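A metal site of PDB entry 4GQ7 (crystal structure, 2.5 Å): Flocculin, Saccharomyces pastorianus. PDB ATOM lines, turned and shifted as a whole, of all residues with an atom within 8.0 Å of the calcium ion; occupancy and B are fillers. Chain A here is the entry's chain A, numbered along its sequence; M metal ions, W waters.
Five residues have an atom within 4 Å of the calcium ion: Asp 112, Asp 113, Asn 176, Lys 178 and Leu 180.
The calcium ion is bound by O of Lys 178 (2.3 Å), OD1 of Asp 113 (2.5 Å), O of Leu 180 (2.5 Å), OD1 of Asn 176 (2.5 Å), OD1 of Asp 112 (2.6 Å) and water W1 (2.6 Å).
N of Lys 178 lies within hydrogen-bond range of O of Thr 86 (2.7 Å). The backbone NH (N) of Ala 177 lies within hydrogen-bond range of the side-chain carboxylate (OD2) of Asp 113 (2.9 Å). OD2 of Asp 113 lies within hydrogen-bond range of OH of Tyr 33, at 2.7 Å. The backbone NH (N) of Asp 113 sits at hydrogen-bond distance from the backbone carbonyl oxygen (O) of Ser 175. The side-chain amide nitrogen (ND2) of Asn 176 sits at hydrogen-bond distance from the backbone carbonyl oxygen (O) of Ala 179 (3.5 Å). The backbone carbonyl oxygen (O) of Pro 85 sits at hydrogen-bond distance from the side-chain amide nitrogen (ND2) of Asn 176, 2.7 Å away. OD2 of Asp 112 is in salt-bridge range of NE of Arg 182 (2.8 Å).
Water W1 bridges OD2 of Asp 112 (2.8 Å) and N of Leu 180 (3.3 Å).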
ATOM      1  N   TYR A  33       4.199 -30.525  16.690  1.00  0.00           N
ATOM      2  CA  TYR A  33       4.621 -31.492  15.667  1.00  0.00           C
ATOM      3  C   TYR A  33       6.029 -32.072  15.857  1.00  0.00           C
ATOM      4  O   TYR A  33       6.512 -32.809  14.997  1.00  0.00           O
ATOM      5  CB  TYR A  33       4.463 -30.932  14.235  1.00  0.00           C
ATOM      6  CG  TYR A  33       5.186 -29.638  13.896  1.00  0.00           C
ATOM      7  CD1 TYR A  33       6.410 -29.299  14.475  1.00  0.00           C
ATOM      8  CD2 TYR A  33       4.643 -28.761  12.954  1.00  0.00           C
ATOM      9  CE1 TYR A  33       7.057 -28.119  14.140  1.00  0.00           C
ATOM     10  CE2 TYR A  33       5.285 -27.581  12.610  1.00  0.00           C
ATOM     11  CZ  TYR A  33       6.493 -27.270  13.207  1.00  0.00           C
ATOM     12  OH  TYR A  33       7.121 -26.088  12.858  1.00  0.00           O
ATOM     13  N   TYR A  62       4.055 -26.239  -1.638  1.00  0.00           N
ATOM     14  CA  TYR A  62       3.369 -24.942  -1.562  1.00  0.00           C
ATOM     15  C   TYR A  62       4.310 -23.838  -1.095  1.00  0.00           C
ATOM     16  O   TYR A  62       5.199 -24.045  -0.269  1.00  0.00           O
ATOM     17  CB  TYR A  62       2.156 -25.013  -0.631  1.00  0.00           C
ATOM     18  CG  TYR A  62       1.423 -23.691  -0.497  1.00  0.00           C
ATOM     19  CD1 TYR A  62       0.577 -23.251  -1.508  1.00  0.00           C
ATOM     20  CD2 TYR A  62       1.593 -22.884   0.619  1.00  0.00           C
ATOM     21  CE1 TYR A  62      -0.085 -22.036  -1.412  1.00  0.00           C
ATOM     22  CE2 TYR A  62       0.927 -21.668   0.728  1.00  0.00           C
ATOM     23  CZ  TYR A  62       0.088 -21.249  -0.287  1.00  0.00           C
ATOM     24  OH  TYR A  62      -0.579 -20.044  -0.199  1.00  0.00           O
ATOM     25  N   PRO A  64       3.678 -19.463  -0.251  1.00  0.00           N
ATOM     26  CA  PRO A  64       2.783 -18.303  -0.341  1.00  0.00           C
ATOM     27  C   PRO A  64       3.392 -17.131  -1.128  1.00  0.00           C
ATOM     28  O   PRO A  64       4.484 -17.271  -1.700  1.00  0.00           O
ATOM     29  CB  PRO A  64       2.561 -17.915   1.131  1.00  0.00           C
ATOM     30  CG  PRO A  64       3.282 -18.921   1.960  1.00  0.00           C
ATOM     31  CD  PRO A  64       4.288 -19.573   1.074  1.00  0.00           C
ATOM     32  N   PRO A  85      -2.128 -24.176   3.756  1.00  0.00           N
ATOM     33  CA  PRO A  85      -0.891 -24.968   3.737  1.00  0.00           C
ATOM     34  C   PRO A  85       0.219 -24.389   4.624  1.00  0.00           C
ATOM     35  O   PRO A  85       1.147 -25.124   4.984  1.00  0.00           O
ATOM     36  CB  PRO A  85      -0.471 -24.931   2.264  1.00  0.00           C
ATOM     37  CG  PRO A  85      -1.711 -24.631   1.503  1.00  0.00           C
ATOM     38  CD  PRO A  85      -2.494 -23.727   2.404  1.00  0.00           C
ATOM     39  N   THR A  86       0.111 -23.106   4.958  1.00  0.00           N
ATOM     40  CA  THR A  86       1.039 -22.461   5.893  1.00  0.00           C
ATOM     41  C   THR A  86       0.892 -23.015   7.298  1.00  0.00           C
ATOM     42  O   THR A  86       1.821 -22.925   8.099  1.00  0.00           O
ATOM     43  CB  THR A  86       0.827 -20.934   5.971  1.00  0.00           C
ATOM     44  OG1 THR A  86      -0.564 -20.665   6.236  1.00  0.00           O
ATOM     45  CG2 THR A  86       1.235 -20.259   4.683  1.00  0.00           C
ATOM     46  N   ASN A  87      -0.299 -23.545   7.606  1.00  0.00           N
ATOM     47  CA  ASN A  87      -0.534 -24.185   8.897  1.00  0.00           C
ATOM     48  C   ASN A  87      -1.624 -25.256   8.842  1.00  0.00           C
ATOM     49  O   ASN A  87      -2.814 -24.951   8.828  1.00  0.00           O
ATOM     50  CB  ASN A  87      -0.838 -23.147   9.963  1.00  0.00           C
ATOM     51  CG  ASN A  87      -1.992 -22.223   9.585  1.00  0.00           C
ATOM     52  OD1 ASN A  87      -1.905 -21.482   8.604  1.00  0.00           O
ATOM     53  ND2 ASN A  87      -3.069 -22.269  10.381  1.00  0.00           N
ATOM     54  N   VAL A 111      12.184 -31.976   4.431  1.00  0.00           N
ATOM     55  CA  VAL A 111      10.987 -31.960   5.288  1.00  0.00           C
ATOM     56  C   VAL A 111      10.764 -30.561   5.862  1.00  0.00           C
ATOM     57  O   VAL A 111      11.658 -29.991   6.476  1.00  0.00           O
ATOM     58  CB  VAL A 111      11.111 -32.966   6.450  1.00  0.00           C
ATOM     59  CG1 VAL A 111       9.877 -32.906   7.337  1.00  0.00           C
ATOM     60  CG2 VAL A 111      11.315 -34.383   5.908  1.00  0.00           C
ATOM     61  N   ASP A 112       9.558 -30.029   5.659  1.00  0.00           N
ATOM     62  CA  ASP A 112       9.272 -28.630   5.974  1.00  0.00           C
ATOM     63  C   ASP A 112       7.751 -28.461   6.224  1.00  0.00           C
ATOM     64  O   ASP A 112       7.005 -28.260   5.259  1.00  0.00           O
ATOM     65  CB  ASP A 112       9.736 -27.777   4.783  1.00  0.00           C
ATOM     66  CG  ASP A 112       9.458 -26.292   4.961  1.00  0.00           C
ATOM     67  OD1 ASP A 112       9.165 -25.847   6.078  1.00  0.00           O
ATOM     68  OD2 ASP A 112       9.526 -25.561   3.945  1.00  0.00           O
ATOM     69  N   ASP A 113       7.290 -28.499   7.483  1.00  0.00           N
ATOM     70  CA  ASP A 113       8.119 -28.470   8.701  1.00  0.00           C
ATOM     71  C   ASP A 113       8.453 -29.840   9.281  1.00  0.00           C
ATOM     72  O   ASP A 113       9.619 -30.115   9.598  1.00  0.00           O
ATOM     73  CB  ASP A 113       7.413 -27.668   9.797  1.00  0.00           C
ATOM     74  CG  ASP A 113       7.364 -26.174   9.513  1.00  0.00           C
ATOM     75  OD1 ASP A 113       8.033 -25.705   8.560  1.00  0.00           O
ATOM     76  OD2 ASP A 113       6.650 -25.461  10.253  1.00  0.00           O
ATOM     77  N   SER A 114       7.428 -30.680   9.466  1.00  0.00           N
ATOM     78  CA  SER A 114       7.590 -31.962  10.155  1.00  0.00           C
ATOM     79  C   SER A 114       6.803 -33.056   9.433  1.00  0.00           C
ATOM     80  O   SER A 114       5.722 -32.794   8.906  1.00  0.00           O
ATOM     81  CB  SER A 114       7.107 -31.852  11.608  1.00  0.00           C
ATOM     82  OG  SER A 114       7.424 -33.005  12.378  1.00  0.00           O
ATOM     83  N   LYS A 146      10.308 -32.675  13.155  1.00  0.00           N
ATOM     84  CA  LYS A 146      11.068 -31.428  13.099  1.00  0.00           C
ATOM     85  C   LYS A 146      12.125 -31.351  14.204  1.00  0.00           C
ATOM     86  O   LYS A 146      11.770 -31.411  15.387  1.00  0.00           O
ATOM     87  CB  LYS A 146      10.133 -30.210  13.165  1.00  0.00           C
ATOM     88  CG  LYS A 146      10.860 -28.877  13.183  1.00  0.00           C
ATOM     89  CD  LYS A 146      10.099 -27.764  12.477  1.00  0.00           C
ATOM     90  CE  LYS A 146      10.461 -26.396  13.014  1.00  0.00           C
ATOM     91  NZ  LYS A 146      11.919 -26.105  12.905  1.00  0.00           N
ATOM     92  N   TYR A 174       2.162 -35.404   7.777  1.00  0.00           N
ATOM     93  CA  TYR A 174       2.949 -34.203   7.539  1.00  0.00           C
ATOM     94  C   TYR A 174       2.299 -33.015   8.222  1.00  0.00           C
ATOM     95  O   TYR A 174       1.073 -32.916   8.290  1.00  0.00           O
ATOM     96  CB  TYR A 174       3.056 -33.950   6.025  1.00  0.00           C
ATOM     97  CG  TYR A 174       3.503 -32.541   5.693  1.00  0.00           C
ATOM     98  CD1 TYR A 174       2.564 -31.519   5.567  1.00  0.00           C
ATOM     99  CD2 TYR A 174       4.835 -32.240   5.535  1.00  0.00           C
ATOM    100  CE1 TYR A 174       2.965 -30.216   5.278  1.00  0.00           C
ATOM    101  CE2 TYR A 174       5.244 -30.948   5.241  1.00  0.00           C
ATOM    102  CZ  TYR A 174       4.304 -29.945   5.116  1.00  0.00           C
ATOM    103  OH  TYR A 174       4.707 -28.672   4.837  1.00  0.00           O
ATOM    104  N   SER A 175       3.121 -32.089   8.734  1.00  0.00           N
ATOM    105  CA  SER A 175       2.618 -30.865   9.344  1.00  0.00           C
ATOM    106  C   SER A 175       3.452 -29.642   8.971  1.00  0.00           C
ATOM    107  O   SER A 175       4.659 -29.743   8.756  1.00  0.00           O
ATOM    108  CB  SER A 175       2.568 -31.023  10.864  1.00  0.00           C
ATOM    109  OG  SER A 175       1.740 -30.023  11.432  1.00  0.00           O
ATOM    110  N   ASN A 176       2.784 -28.491   8.890  1.00  0.00           N
ATOM    111  CA  ASN A 176       3.440 -27.209   8.664  1.00  0.00           C
ATOM    112  C   ASN A 176       2.880 -26.172   9.623  1.00  0.00           C
ATOM    113  O   ASN A 176       1.708 -26.221   9.963  1.00  0.00           O
ATOM    114  CB  ASN A 176       3.187 -26.752   7.221  1.00  0.00           C
ATOM    115  CG  ASN A 176       4.116 -25.629   6.788  1.00  0.00           C
ATOM    116  OD1 ASN A 176       5.221 -25.461   7.300  1.00  0.00           O
ATOM    117  ND2 ASN A 176       3.659 -24.840   5.812  1.00  0.00           N
ATOM    118  N   ALA A 177       3.735 -25.270  10.095  1.00  0.00           N
ATOM    119  CA  ALA A 177       3.331 -24.198  10.999  1.00  0.00           C
ATOM    120  C   ALA A 177       3.492 -22.812  10.373  1.00  0.00           C
ATOM    121  O   ALA A 177       2.958 -21.838  10.905  1.00  0.00           O
ATOM    122  CB  ALA A 177       4.147 -24.267  12.278  1.00  0.00           C
ATOM    123  N   LYS A 178       4.232 -22.714   9.278  1.00  0.00           N
ATOM    124  CA  LYS A 178       4.610 -21.415   8.743  1.00  0.00           C
ATOM    125  C   LYS A 178       5.104 -21.515   7.308  1.00  0.00           C
ATOM    126  O   LYS A 178       5.778 -22.476   6.941  1.00  0.00           O
ATOM    127  CB  LYS A 178       5.739 -20.829   9.598  1.00  0.00           C
ATOM    128  CG  LYS A 178       5.765 -19.304   9.635  1.00  0.00           C
ATOM    129  CD  LYS A 178       7.168 -18.758   9.882  1.00  0.00           C
ATOM    130  CE  LYS A 178       7.872 -19.442  11.038  1.00  0.00           C
ATOM    131  NZ  LYS A 178       8.991 -18.603  11.555  1.00  0.00           N
ATOM    132  N   ALA A 179       4.757 -20.500   6.505  1.00  0.00           N
ATOM    133  CA  ALA A 179       5.375 -20.256   5.204  1.00  0.00           C
ATOM    134  C   ALA A 179       5.324 -21.451   4.246  1.00  0.00           C
ATOM    135  O   ALA A 179       4.237 -21.965   3.975  1.00  0.00           O
ATOM    136  CB  ALA A 179       6.815 -19.754   5.398  1.00  0.00           C
ATOM    137  N   LEU A 180       6.479 -21.896   3.749  1.00  0.00           N
ATOM    138  CA  LEU A 180       6.559 -22.982   2.760  1.00  0.00           C
ATOM    139  C   LEU A 180       6.093 -24.313   3.327  1.00  0.00           C
ATOM    140  O   LEU A 180       6.296 -24.612   4.507  1.00  0.00           O
ATOM    141  CB  LEU A 180       8.007 -23.152   2.256  1.00  0.00           C
ATOM    142  CG  LEU A 180       8.554 -22.233   1.171  1.00  0.00           C
ATOM    143  CD1 LEU A 180       8.201 -20.780   1.408  1.00  0.00           C
ATOM    144  CD2 LEU A 180      10.067 -22.388   1.059  1.00  0.00           C
ATOM    145  N   ALA A 181       5.458 -25.103   2.468  1.00  0.00           N
ATOM    146  CA  ALA A 181       5.148 -26.494   2.754  1.00  0.00           C
ATOM    147  C   ALA A 181       5.863 -27.346   1.709  1.00  0.00           C
ATOM    148  O   ALA A 181       5.565 -27.260   0.518  1.00  0.00           O
ATOM    149  CB  ALA A 181       3.649 -26.746   2.684  1.00  0.00           C
ATOM    150  N   ARG A 182       6.807 -28.160   2.161  1.00  0.00           N
ATOM    151  CA  ARG A 182       7.628 -28.977   1.276  1.00  0.00           C
ATOM    152  C   ARG A 182       7.829 -30.377   1.821  1.00  0.00           C
ATOM    153  O   ARG A 182       8.460 -30.566   2.866  1.00  0.00           O
ATOM    154  CB  ARG A 182       9.012 -28.351   1.064  1.00  0.00           C
ATOM    155  CG  ARG A 182       8.991 -26.990   0.395  1.00  0.00           C
ATOM    156  CD  ARG A 182      10.400 -26.434   0.270  1.00  0.00           C
ATOM    157  NE  ARG A 182      10.909 -26.013   1.578  1.00  0.00           N
ATOM    158  CZ  ARG A 182      12.188 -25.965   1.922  1.00  0.00           C
ATOM    159  NH1 ARG A 182      13.154 -26.312   1.074  1.00  0.00           N
ATOM    160  NH2 ARG A 182      12.524 -25.562   3.137  1.00  0.00           N
HETATM  161 CA    CA M   1       7.326 -24.183   6.761  1.00  0.00          CA
HETATM  162  O   HOH W   1       9.182 -23.077   5.293  1.00  0.00           O
